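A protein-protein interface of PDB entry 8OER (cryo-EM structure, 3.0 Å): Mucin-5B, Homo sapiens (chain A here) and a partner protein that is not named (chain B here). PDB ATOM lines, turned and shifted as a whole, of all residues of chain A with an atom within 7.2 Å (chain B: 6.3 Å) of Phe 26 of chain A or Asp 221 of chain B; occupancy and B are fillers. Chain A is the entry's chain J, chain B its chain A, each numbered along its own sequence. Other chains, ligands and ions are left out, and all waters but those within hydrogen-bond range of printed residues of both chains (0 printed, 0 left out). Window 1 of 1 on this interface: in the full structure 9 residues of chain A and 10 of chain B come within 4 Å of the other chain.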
ATOM      1  N   GLY A  14     -19.079   9.222  15.411  1.00  0.00           N
ATOM      2  CA  GLY A  14     -19.226  10.037  16.601  1.00  0.00           C
ATOM      3  C   GLY A  14     -20.438  10.940  16.620  1.00  0.00           C
ATOM      4  O   GLY A  14     -20.603  11.731  17.552  1.00  0.00           O
ATOM      5  N   HIS A  15     -21.293  10.847  15.606  1.00  0.00           N
ATOM      6  CA  HIS A  15     -22.478  11.686  15.542  1.00  0.00           C
ATOM      7  C   HIS A  15     -23.566  10.999  14.732  1.00  0.00           C
ATOM      8  O   HIS A  15     -23.287  10.212  13.824  1.00  0.00           O
ATOM      9  CB  HIS A  15     -22.158  13.057  14.929  1.00  0.00           C
ATOM     10  CG  HIS A  15     -23.223  14.086  15.149  1.00  0.00           C
ATOM     11  ND1 HIS A  15     -23.531  14.586  16.396  1.00  0.00           N
ATOM     12  CD2 HIS A  15     -24.046  14.715  14.280  1.00  0.00           C
ATOM     13  CE1 HIS A  15     -24.501  15.475  16.285  1.00  0.00           C
ATOM     14  NE2 HIS A  15     -24.831  15.573  15.010  1.00  0.00           N
ATOM     15  N   PRO A  17     -26.449  12.451  12.360  1.00  0.00           N
ATOM     16  CA  PRO A  17     -26.916  13.712  11.774  1.00  0.00           C
ATOM     17  C   PRO A  17     -28.392  13.951  12.051  1.00  0.00           C
ATOM     18  O   PRO A  17     -29.198  13.020  12.094  1.00  0.00           O
ATOM     19  CB  PRO A  17     -26.642  13.531  10.276  1.00  0.00           C
ATOM     20  CG  PRO A  17     -26.432  12.068  10.092  1.00  0.00           C
ATOM     21  CD  PRO A  17     -25.844  11.566  11.356  1.00  0.00           C
ATOM     22  N   LEU A  21     -32.564  21.855   8.391  1.00  0.00           N
ATOM     23  CA  LEU A  21     -31.797  22.649   7.436  1.00  0.00           C
ATOM     24  C   LEU A  21     -30.369  22.913   7.892  1.00  0.00           C
ATOM     25  O   LEU A  21     -29.459  22.965   7.059  1.00  0.00           O
ATOM     26  CB  LEU A  21     -32.502  23.981   7.167  1.00  0.00           C
ATOM     27  CG  LEU A  21     -33.701  23.929   6.216  1.00  0.00           C
ATOM     28  CD1 LEU A  21     -34.376  25.287   6.129  1.00  0.00           C
ATOM     29  CD2 LEU A  21     -33.276  23.446   4.839  1.00  0.00           C
ATOM     30  N   GLY A  22     -30.149  23.088   9.193  1.00  0.00           N
ATOM     31  CA  GLY A  22     -28.818  23.328   9.710  1.00  0.00           C
ATOM     32  C   GLY A  22     -28.121  22.125  10.287  1.00  0.00           C
ATOM     33  O   GLY A  22     -26.928  22.198  10.596  1.00  0.00           O
ATOM     34  N   GLY A  23     -28.831  21.014  10.444  1.00  0.00           N
ATOM     35  CA  GLY A  23     -28.233  19.806  10.960  1.00  0.00           C
ATOM     36  C   GLY A  23     -27.373  19.121   9.924  1.00  0.00           C
ATOM     37  O   GLY A  23     -27.325  19.495   8.754  1.00  0.00           O
ATOM     38  N   GLY A  24     -26.681  18.094  10.371  1.00  0.00           N
ATOM     39  CA  GLY A  24     -25.783  17.359   9.511  1.00  0.00           C
ATOM     40  C   GLY A  24     -24.819  16.544  10.343  1.00  0.00           C
ATOM     41  O   GLY A  24     -25.022  16.336  11.535  1.00  0.00           O
ATOM     42  N   ASP A  25     -23.759  16.092   9.687  1.00  0.00           N
ATOM     43  CA  ASP A  25     -22.767  15.227  10.313  1.00  0.00           C
ATOM     44  C   ASP A  25     -21.411  15.910  10.255  1.00  0.00           C
ATOM     45  O   ASP A  25     -20.867  16.119   9.167  1.00  0.00           O
ATOM     46  CB  ASP A  25     -22.719  13.862   9.627  1.00  0.00           C
ATOM     47  CG  ASP A  25     -22.262  12.761  10.558  1.00  0.00           C
ATOM     48  OD1 ASP A  25     -21.861  13.077  11.696  1.00  0.00           O
ATOM     49  OD2 ASP A  25     -22.311  11.580  10.159  1.00  0.00           O
ATOM     50  N   PHE A  26     -20.868  16.253  11.422  1.00  0.00           N
ATOM     51  CA  PHE A  26     -19.612  16.998  11.515  1.00  0.00           C
ATOM     52  C   PHE A  26     -18.626  16.182  12.344  1.00  0.00           C
ATOM     53  O   PHE A  26     -18.486  16.391  13.551  1.00  0.00           O
ATOM     54  CB  PHE A  26     -19.848  18.375  12.118  1.00  0.00           C
ATOM     55  CG  PHE A  26     -20.388  19.375  11.140  1.00  0.00           C
ATOM     56  CD1 PHE A  26     -19.548  20.002  10.235  1.00  0.00           C
ATOM     57  CD2 PHE A  26     -21.737  19.689  11.124  1.00  0.00           C
ATOM     58  CE1 PHE A  26     -20.040  20.920   9.335  1.00  0.00           C
ATOM     59  CE2 PHE A  26     -22.236  20.607  10.228  1.00  0.00           C
ATOM     60  CZ  PHE A  26     -21.386  21.224   9.332  1.00  0.00           C
ATOM     61  N   GLU A  27     -17.923  15.265  11.685  1.00  0.00           N
ATOM     62  CA  GLU A  27     -16.949  14.409  12.352  1.00  0.00           C
ATOM     63  C   GLU A  27     -15.609  15.124  12.292  1.00  0.00           C
ATOM     64  O   GLU A  27     -14.853  14.993  11.329  1.00  0.00           O
ATOM     65  CB  GLU A  27     -16.890  13.043  11.681  1.00  0.00           C
ATOM     66  CG  GLU A  27     -18.210  12.287  11.626  1.00  0.00           C
ATOM     67  CD  GLU A  27     -18.745  11.917  12.996  1.00  0.00           C
ATOM     68  OE1 GLU A  27     -17.955  11.879  13.962  1.00  0.00           O
ATOM     69  OE2 GLU A  27     -19.958  11.642  13.103  1.00  0.00           O
ATOM     70  N   THR A  28     -15.311  15.901  13.327  1.00  0.00           N
ATOM     71  CA  THR A  28     -14.118  16.732  13.358  1.00  0.00           C
ATOM     72  C   THR A  28     -13.115  16.190  14.368  1.00  0.00           C
ATOM     73  O   THR A  28     -13.490  15.625  15.397  1.00  0.00           O
ATOM     74  CB  THR A  28     -14.471  18.181  13.698  1.00  0.00           C
ATOM     75  OG1 THR A  28     -14.462  18.354  15.119  1.00  0.00           O
ATOM     76  CG2 THR A  28     -15.854  18.529  13.156  1.00  0.00           C
ATOM     77  N   PHE A  29     -11.828  16.378  14.058  1.00  0.00           N
ATOM     78  CA  PHE A  29     -10.772  15.792  14.881  1.00  0.00           C
ATOM     79  C   PHE A  29     -10.822  16.315  16.310  1.00  0.00           C
ATOM     80  O   PHE A  29     -10.714  15.539  17.268  1.00  0.00           O
ATOM     81  CB  PHE A  29      -9.398  16.073  14.268  1.00  0.00           C
ATOM     82  CG  PHE A  29      -9.160  15.396  12.946  1.00  0.00           C
ATOM     83  CD1 PHE A  29     -10.056  14.466  12.445  1.00  0.00           C
ATOM     84  CD2 PHE A  29      -8.026  15.687  12.206  1.00  0.00           C
ATOM     85  CE1 PHE A  29      -9.826  13.848  11.228  1.00  0.00           C
ATOM     86  CE2 PHE A  29      -7.793  15.071  10.991  1.00  0.00           C
ATOM     87  CZ  PHE A  29      -8.694  14.152  10.503  1.00  0.00           C
ATOM     88  N   ASN A  31     -13.408  17.600  17.892  1.00  0.00           N
ATOM     89  CA  ASN A  31     -14.587  17.040  18.544  1.00  0.00           C
ATOM     90  C   ASN A  31     -14.358  15.587  18.935  1.00  0.00           C
ATOM     91  O   ASN A  31     -14.810  15.146  19.998  1.00  0.00           O
ATOM     92  CB  ASN A  31     -15.816  17.170  17.646  1.00  0.00           C
ATOM     93  CG  ASN A  31     -16.902  16.164  17.992  1.00  0.00           C
ATOM     94  OD1 ASN A  31     -16.836  14.993  17.611  1.00  0.00           O
ATOM     95  ND2 ASN A  31     -17.892  16.611  18.754  1.00  0.00           N
ATOM     96  N   LEU A  32     -13.671  14.824  18.082  1.00  0.00           N
ATOM     97  CA  LEU A  32     -13.359  13.442  18.425  1.00  0.00           C
ATOM     98  C   LEU A  32     -12.482  13.375  19.667  1.00  0.00           C
ATOM     99  O   LEU A  32     -12.685  12.517  20.535  1.00  0.00           O
ATOM    100  CB  LEU A  32     -12.682  12.745  17.245  1.00  0.00           C
ATOM    101  CG  LEU A  32     -13.573  12.238  16.106  1.00  0.00           C
ATOM    102  CD1 LEU A  32     -12.879  11.124  15.331  1.00  0.00           C
ATOM    103  CD2 LEU A  32     -14.923  11.772  16.624  1.00  0.00           C
ATOM    104  N   ASP A  66     -17.521  16.815   2.435  1.00  0.00           N
ATOM    105  CA  ASP A  66     -16.107  17.116   2.264  1.00  0.00           C
ATOM    106  C   ASP A  66     -15.304  16.494   3.395  1.00  0.00           C
ATOM    107  O   ASP A  66     -15.543  16.793   4.568  1.00  0.00           O
ATOM    108  CB  ASP A  66     -15.863  18.627   2.207  1.00  0.00           C
ATOM    109  CG  ASP A  66     -16.773  19.401   3.135  1.00  0.00           C
ATOM    110  OD1 ASP A  66     -16.723  20.649   3.124  1.00  0.00           O
ATOM    111  OD2 ASP A  66     -17.549  18.761   3.866  1.00  0.00           O
ATOM    112  N   ARG A  71      -8.550  17.843   8.725  1.00  0.00           N
ATOM    113  CA  ARG A  71      -9.581  18.528   9.492  1.00  0.00           C
ATOM    114  C   ARG A  71     -10.805  17.671   9.792  1.00  0.00           C
ATOM    115  O   ARG A  71     -11.397  17.828  10.862  1.00  0.00           O
ATOM    116  CB  ARG A  71      -9.940  19.818   8.736  1.00  0.00           C
ATOM    117  CG  ARG A  71     -10.837  20.796   9.460  1.00  0.00           C
ATOM    118  CD  ARG A  71     -11.517  21.704   8.448  1.00  0.00           C
ATOM    119  NE  ARG A  71     -11.837  23.025   8.975  1.00  0.00           N
ATOM    120  CZ  ARG A  71     -12.781  23.269   9.873  1.00  0.00           C
ATOM    121  NH1 ARG A  71     -13.521  22.298  10.380  1.00  0.00           N
ATOM    122  NH2 ARG A  71     -12.992  24.521  10.268  1.00  0.00           N
ATOM    123  N   GLY A  72     -11.200  16.761   8.886  1.00  0.00           N
ATOM    124  CA  GLY A  72     -12.266  15.832   9.204  1.00  0.00           C
ATOM    125  C   GLY A  72     -13.302  15.750   8.098  1.00  0.00           C
ATOM    126  O   GLY A  72     -13.024  16.057   6.933  1.00  0.00           O
ATOM    127  N   LEU A  73     -14.513  15.322   8.470  1.00  0.00           N
ATOM    128  CA  LEU A  73     -15.612  15.079   7.540  1.00  0.00           C
ATOM    129  C   LEU A  73     -16.776  16.004   7.863  1.00  0.00           C
ATOM    130  O   LEU A  73     -17.171  16.124   9.026  1.00  0.00           O
ATOM    131  CB  LEU A  73     -16.069  13.612   7.602  1.00  0.00           C
ATOM    132  CG  LEU A  73     -17.420  13.158   7.021  1.00  0.00           C
ATOM    133  CD1 LEU A  73     -17.365  11.687   6.680  1.00  0.00           C
ATOM    134  CD2 LEU A  73     -18.582  13.377   7.972  1.00  0.00           C
ATOM    135  N   MET A  74     -17.331  16.647   6.836  1.00  0.00           N
ATOM    136  CA  MET A  74     -18.481  17.520   7.021  1.00  0.00           C
ATOM    137  C   MET A  74     -19.571  17.206   6.008  1.00  0.00           C
ATOM    138  O   MET A  74     -19.290  16.956   4.830  1.00  0.00           O
ATOM    139  CB  MET A  74     -18.117  19.002   6.892  1.00  0.00           C
ATOM    140  CG  MET A  74     -17.056  19.483   7.840  1.00  0.00           C
ATOM    141  SD  MET A  74     -15.431  18.821   7.469  1.00  0.00           S
ATOM    142  CE  MET A  74     -14.446  20.177   8.053  1.00  0.00           C
ATOM    143  N   CYS A  75     -20.814  17.231   6.486  1.00  0.00           N
ATOM    144  CA  CYS A  75     -22.006  17.171   5.649  1.00  0.00           C
ATOM    145  C   CYS A  75     -23.048  18.098   6.251  1.00  0.00           C
ATOM    146  O   CYS A  75     -23.479  17.885   7.389  1.00  0.00           O
ATOM    147  CB  CYS A  75     -22.558  15.745   5.559  1.00  0.00           C
ATOM    148  SG  CYS A  75     -23.931  15.518   4.391  1.00  0.00           S
ATOM    149  N   ALA A  76     -23.455  19.112   5.494  1.00  0.00           N
ATOM    150  CA  ALA A  76     -24.505  20.035   5.903  1.00  0.00           C
ATOM    151  C   ALA A  76     -25.785  19.734   5.137  1.00  0.00           C
ATOM    152  O   ALA A  76     -25.746  19.408   3.949  1.00  0.00           O
ATOM    153  CB  ALA A  76     -24.085  21.485   5.669  1.00  0.00           C
ATOM    154  N   ASN A  77     -26.920  19.846   5.827  1.00  0.00           N
ATOM    155  CA  ASN A  77     -28.190  19.453   5.225  1.00  0.00           C
ATOM    156  C   ASN A  77     -28.533  20.318   4.019  1.00  0.00           C
ATOM    157  O   ASN A  77     -29.036  19.814   3.010  1.00  0.00           O
ATOM    158  CB  ASN A  77     -29.308  19.530   6.265  1.00  0.00           C
ATOM    159  CG  ASN A  77     -29.650  18.179   6.847  1.00  0.00           C
ATOM    160  OD1 ASN A  77     -28.859  17.242   6.770  1.00  0.00           O
ATOM    161  ND2 ASN A  77     -30.837  18.069   7.431  1.00  0.00           N
ATOM    162  N   LEU A  90     -15.535   7.781   9.701  1.00  0.00           N
ATOM    163  CA  LEU A  90     -14.231   7.748   9.057  1.00  0.00           C
ATOM    164  C   LEU A  90     -13.258   6.934   9.894  1.00  0.00           C
ATOM    165  O   LEU A  90     -13.533   6.581  11.043  1.00  0.00           O
ATOM    166  CB  LEU A  90     -13.661   9.154   8.856  1.00  0.00           C
ATOM    167  CG  LEU A  90     -13.339   9.861  10.169  1.00  0.00           C
ATOM    168  CD1 LEU A  90     -12.073  10.688  10.040  1.00  0.00           C
ATOM    169  CD2 LEU A  90     -14.504  10.725  10.600  1.00  0.00           C
ATOM    170  N   PRO B  71     -23.160  26.882  21.578  1.00  0.00           N
ATOM    171  CA  PRO B  71     -21.694  26.891  21.578  1.00  0.00           C
ATOM    172  C   PRO B  71     -21.081  26.959  20.182  1.00  0.00           C
ATOM    173  O   PRO B  71     -20.111  26.261  19.875  1.00  0.00           O
ATOM    174  CB  PRO B  71     -21.351  25.569  22.270  1.00  0.00           C
ATOM    175  CG  PRO B  71     -22.458  24.664  21.866  1.00  0.00           C
ATOM    176  CD  PRO B  71     -23.698  25.517  21.701  1.00  0.00           C
ATOM    177  N   CYS B  74     -18.116  29.953  14.854  1.00  0.00           N
ATOM    178  CA  CYS B  74     -17.857  30.591  13.571  1.00  0.00           C
ATOM    179  C   CYS B  74     -18.472  31.988  13.564  1.00  0.00           C
ATOM    180  O   CYS B  74     -18.911  32.503  14.593  1.00  0.00           O
ATOM    181  CB  CYS B  74     -18.389  29.735  12.421  1.00  0.00           C
ATOM    182  SG  CYS B  74     -18.622  28.000  12.824  1.00  0.00           S
ATOM    183  N   TYR B  76     -21.476  34.477  12.708  1.00  0.00           N
ATOM    184  CA  TYR B  76     -22.917  34.301  12.714  1.00  0.00           C
ATOM    185  C   TYR B  76     -23.584  35.646  12.505  1.00  0.00           C
ATOM    186  O   TYR B  76     -23.033  36.689  12.859  1.00  0.00           O
ATOM    187  CB  TYR B  76     -23.400  33.673  14.024  1.00  0.00           C
ATOM    188  CG  TYR B  76     -22.973  32.240  14.203  1.00  0.00           C
ATOM    189  CD1 TYR B  76     -21.760  31.931  14.779  1.00  0.00           C
ATOM    190  CD2 TYR B  76     -23.788  31.197  13.804  1.00  0.00           C
ATOM    191  CE1 TYR B  76     -21.358  30.626  14.943  1.00  0.00           C
ATOM    192  CE2 TYR B  76     -23.397  29.890  13.966  1.00  0.00           C
ATOM    193  CZ  TYR B  76     -22.182  29.609  14.536  1.00  0.00           C
ATOM    194  OH  TYR B  76     -21.791  28.303  14.700  1.00  0.00           O
ATOM    195  N   LEU B 204     -29.320  24.647  19.182  1.00  0.00           N
ATOM    196  CA  LEU B 204     -28.194  24.324  18.313  1.00  0.00           C
ATOM    197  C   LEU B 204     -28.579  24.490  16.850  1.00  0.00           C
ATOM    198  O   LEU B 204     -27.868  25.146  16.077  1.00  0.00           O
ATOM    199  CB  LEU B 204     -27.709  22.903  18.580  1.00  0.00           C
ATOM    200  CG  LEU B 204     -26.646  22.438  17.588  1.00  0.00           C
ATOM    201  CD1 LEU B 204     -25.449  23.359  17.648  1.00  0.00           C
ATOM    202  CD2 LEU B 204     -26.235  21.004  17.863  1.00  0.00           C
ATOM    203  N   ASN B 208     -27.451  27.378  14.221  1.00  0.00           N
ATOM    204  CA  ASN B 208     -26.817  26.909  12.998  1.00  0.00           C
ATOM    205  C   ASN B 208     -27.492  27.458  11.751  1.00  0.00           C
ATOM    206  O   ASN B 208     -26.844  27.577  10.709  1.00  0.00           O
ATOM    207  CB  ASN B 208     -26.804  25.384  12.972  1.00  0.00           C
ATOM    208  CG  ASN B 208     -25.705  24.805  13.829  1.00  0.00           C
ATOM    209  OD1 ASN B 208     -24.717  25.476  14.118  1.00  0.00           O
ATOM    210  ND2 ASN B 208     -25.867  23.558  14.245  1.00  0.00           N
ATOM    211  N   LYS B 211     -26.005  31.053  10.288  1.00  0.00           N
ATOM    212  CA  LYS B 211     -24.572  30.867  10.123  1.00  0.00           C
ATOM    213  C   LYS B 211     -24.130  31.497   8.810  1.00  0.00           C
ATOM    214  O   LYS B 211     -24.924  31.642   7.877  1.00  0.00           O
ATOM    215  CB  LYS B 211     -24.213  29.379  10.145  1.00  0.00           C
ATOM    216  CG  LYS B 211     -22.737  29.078  10.293  1.00  0.00           C
ATOM    217  CD  LYS B 211     -22.492  27.581  10.232  1.00  0.00           C
ATOM    218  CE  LYS B 211     -21.056  27.269   9.868  1.00  0.00           C
ATOM    219  NZ  LYS B 211     -20.923  26.974   8.422  1.00  0.00           N
ATOM    220  N   CYS B 219     -16.364  26.306   8.446  1.00  0.00           N
ATOM    221  CA  CYS B 219     -16.363  26.065   9.881  1.00  0.00           C
ATOM    222  C   CYS B 219     -17.423  25.027  10.242  1.00  0.00           C
ATOM    223  O   CYS B 219     -18.545  25.083   9.734  1.00  0.00           O
ATOM    224  CB  CYS B 219     -16.622  27.361  10.642  1.00  0.00           C
ATOM    225  SG  CYS B 219     -16.812  27.172  12.426  1.00  0.00           S
ATOM    226  N   PRO B 220     -17.104  24.081  11.115  1.00  0.00           N
ATOM    227  CA  PRO B 220     -18.077  23.038  11.451  1.00  0.00           C
ATOM    228  C   PRO B 220     -19.185  23.557  12.347  1.00  0.00           C
ATOM    229  O   PRO B 220     -19.269  24.756  12.621  1.00  0.00           O
ATOM    230  CB  PRO B 220     -17.221  21.992  12.172  1.00  0.00           C
ATOM    231  CG  PRO B 220     -16.165  22.802  12.831  1.00  0.00           C
ATOM    232  CD  PRO B 220     -15.846  23.915  11.863  1.00  0.00           C
ATOM    233  N   ASP B 221     -20.044  22.663  12.795  1.00  0.00           N
ATOM    234  CA  ASP B 221     -21.060  23.012  13.762  1.00  0.00           C
ATOM    235  C   ASP B 221     -20.735  22.387  15.109  1.00  0.00           C
ATOM    236  O   ASP B 221     -20.158  21.295  15.160  1.00  0.00           O
ATOM    237  CB  ASP B 221     -22.439  22.537  13.303  1.00  0.00           C
ATOM    238  CG  ASP B 221     -23.025  23.423  12.236  1.00  0.00           C
ATOM    239  OD1 ASP B 221     -22.337  24.374  11.821  1.00  0.00           O
ATOM    240  OD2 ASP B 221     -24.170  23.170  11.813  1.00  0.00           O
ATOM    241  N   PRO B 222     -21.078  23.046  16.214  1.00  0.00           N
ATOM    242  CA  PRO B 222     -20.788  22.474  17.535  1.00  0.00           C
ATOM    243  C   PRO B 222     -21.700  21.291  17.818  1.00  0.00           C
ATOM    244  O   PRO B 222     -22.925  21.425  17.844  1.00  0.00           O
ATOM    245  CB  PRO B 222     -21.057  23.638  18.492  1.00  0.00           C
ATOM    246  CG  PRO B 222     -22.041  24.482  17.774  1.00  0.00           C
ATOM    247  CD  PRO B 222     -21.729  24.363  16.314  1.00  0.00           C
ATOM    248  N   LEU B 223     -21.095  20.126  18.022  1.00  0.00           N
ATOM    249  CA  LEU B 223     -21.865  18.953  18.382  1.00  0.00           C
ATOM    250  C   LEU B 223     -22.436  19.127  19.788  1.00  0.00           C
ATOM    251  O   LEU B 223     -21.802  19.742  20.649  1.00  0.00           O
ATOM    252  CB  LEU B 223     -20.996  17.702  18.305  1.00  0.00           C
ATOM    253  CG  LEU B 223     -20.642  17.268  16.878  1.00  0.00           C
ATOM    254  CD1 LEU B 223     -19.451  18.040  16.320  1.00  0.00           C
ATOM    255  CD2 LEU B 223     -20.388  15.773  16.818  1.00  0.00           C
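Of chain B, only Pro 220 (3.6 Å), Asp 221 (3.5 Å) and Leu 223 (3.4 Å) come within 4 Å of Phe 26 of chain A. Asp 221 of chain B touches two residues of chain A. Printed residues of chain B within 4 Å of Arg 71 of chain A: Cys 219 and Pro 220. Printed residues of chain B within 4 Å of Thr 28 of chain A: Pro 220 (3.9 Å). Of the printed residues of chain A, Leu 223 of chain B touches His 15 (3.4 Å), Phe 26 (3.4 Å) and Asn 31 (3.2 Å). Ala 76 of chain A touches none of the printed residues of chain B. Lys 211 of chain B touches none of the printed residues of chain A. The nearest printed residue of chain B that does not touch Thr 28 of chain A is Leu 223 of chain B (4.8 Å).
The backbone carbonyl oxygen (O) of Gly 22 of chain A lies close to the side-chain carboxylate (OD2) of Asp 221 of chain B (3.2 Å).
Printed residues of chain B that touch a printed residue of chain A: Asn 208, Cys 219, Pro 220, Asp 221 and Leu 223. Of the 23 printed residues of chain A, 6 touch a printed residue of chain B. Hydrophobic or aromatic side chains of chain A that line the printed part of chain B: His 15 and Phe 26. Among the printed residues, no Asp or Glu carboxylate lies within 4 Å of a Lys or Arg side-chain nitrogen of the other chain.
The side-chain sulfur of Cys 219 of chain B forms a disulfide with the side-chain sulfur of Cys 74 of chain B, 2.0 Å away. O of Leu 204 of chain B lies close to ND2 of Asn 208 of chain B (3.1 Å). The side-chain amide nitrogen (ND2) of Asn 208 of chain B sits at hydrogen-bond distance from the side-chain carboxylate (OD2) of Asp 221 of chain B, 3.0 Å away. The side-chain amino group of Lys 211 of chain B is in hydrogen-bond range of the backbone carbonyl oxygen of Cys 219 of chain B, at 3.3 Å. N of Asn 31 of chain A sits at hydrogen-bond distance from OG1 of Thr 28 of chain A (3.1 Å).
Among the printed residues, pairs that only touch across the chains: His 15 of chain A with Leu 223 of chain B, Gly 22 of chain A with Asn 208 of chain B, Phe 26 of chain A with Pro 220 of chain B, Phe 26 of chain A with Asp 221 of chain B, Phe 26 of chain A with Leu 223 of chain B, Thr 28 of chain A with Pro 220 of chain B, Asn 31 of chain A with Leu 223 of chain B, Arg 71 of chain A with Cys 219 of chain B and Arg 71 of chain A with Pro 220 of chain B.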
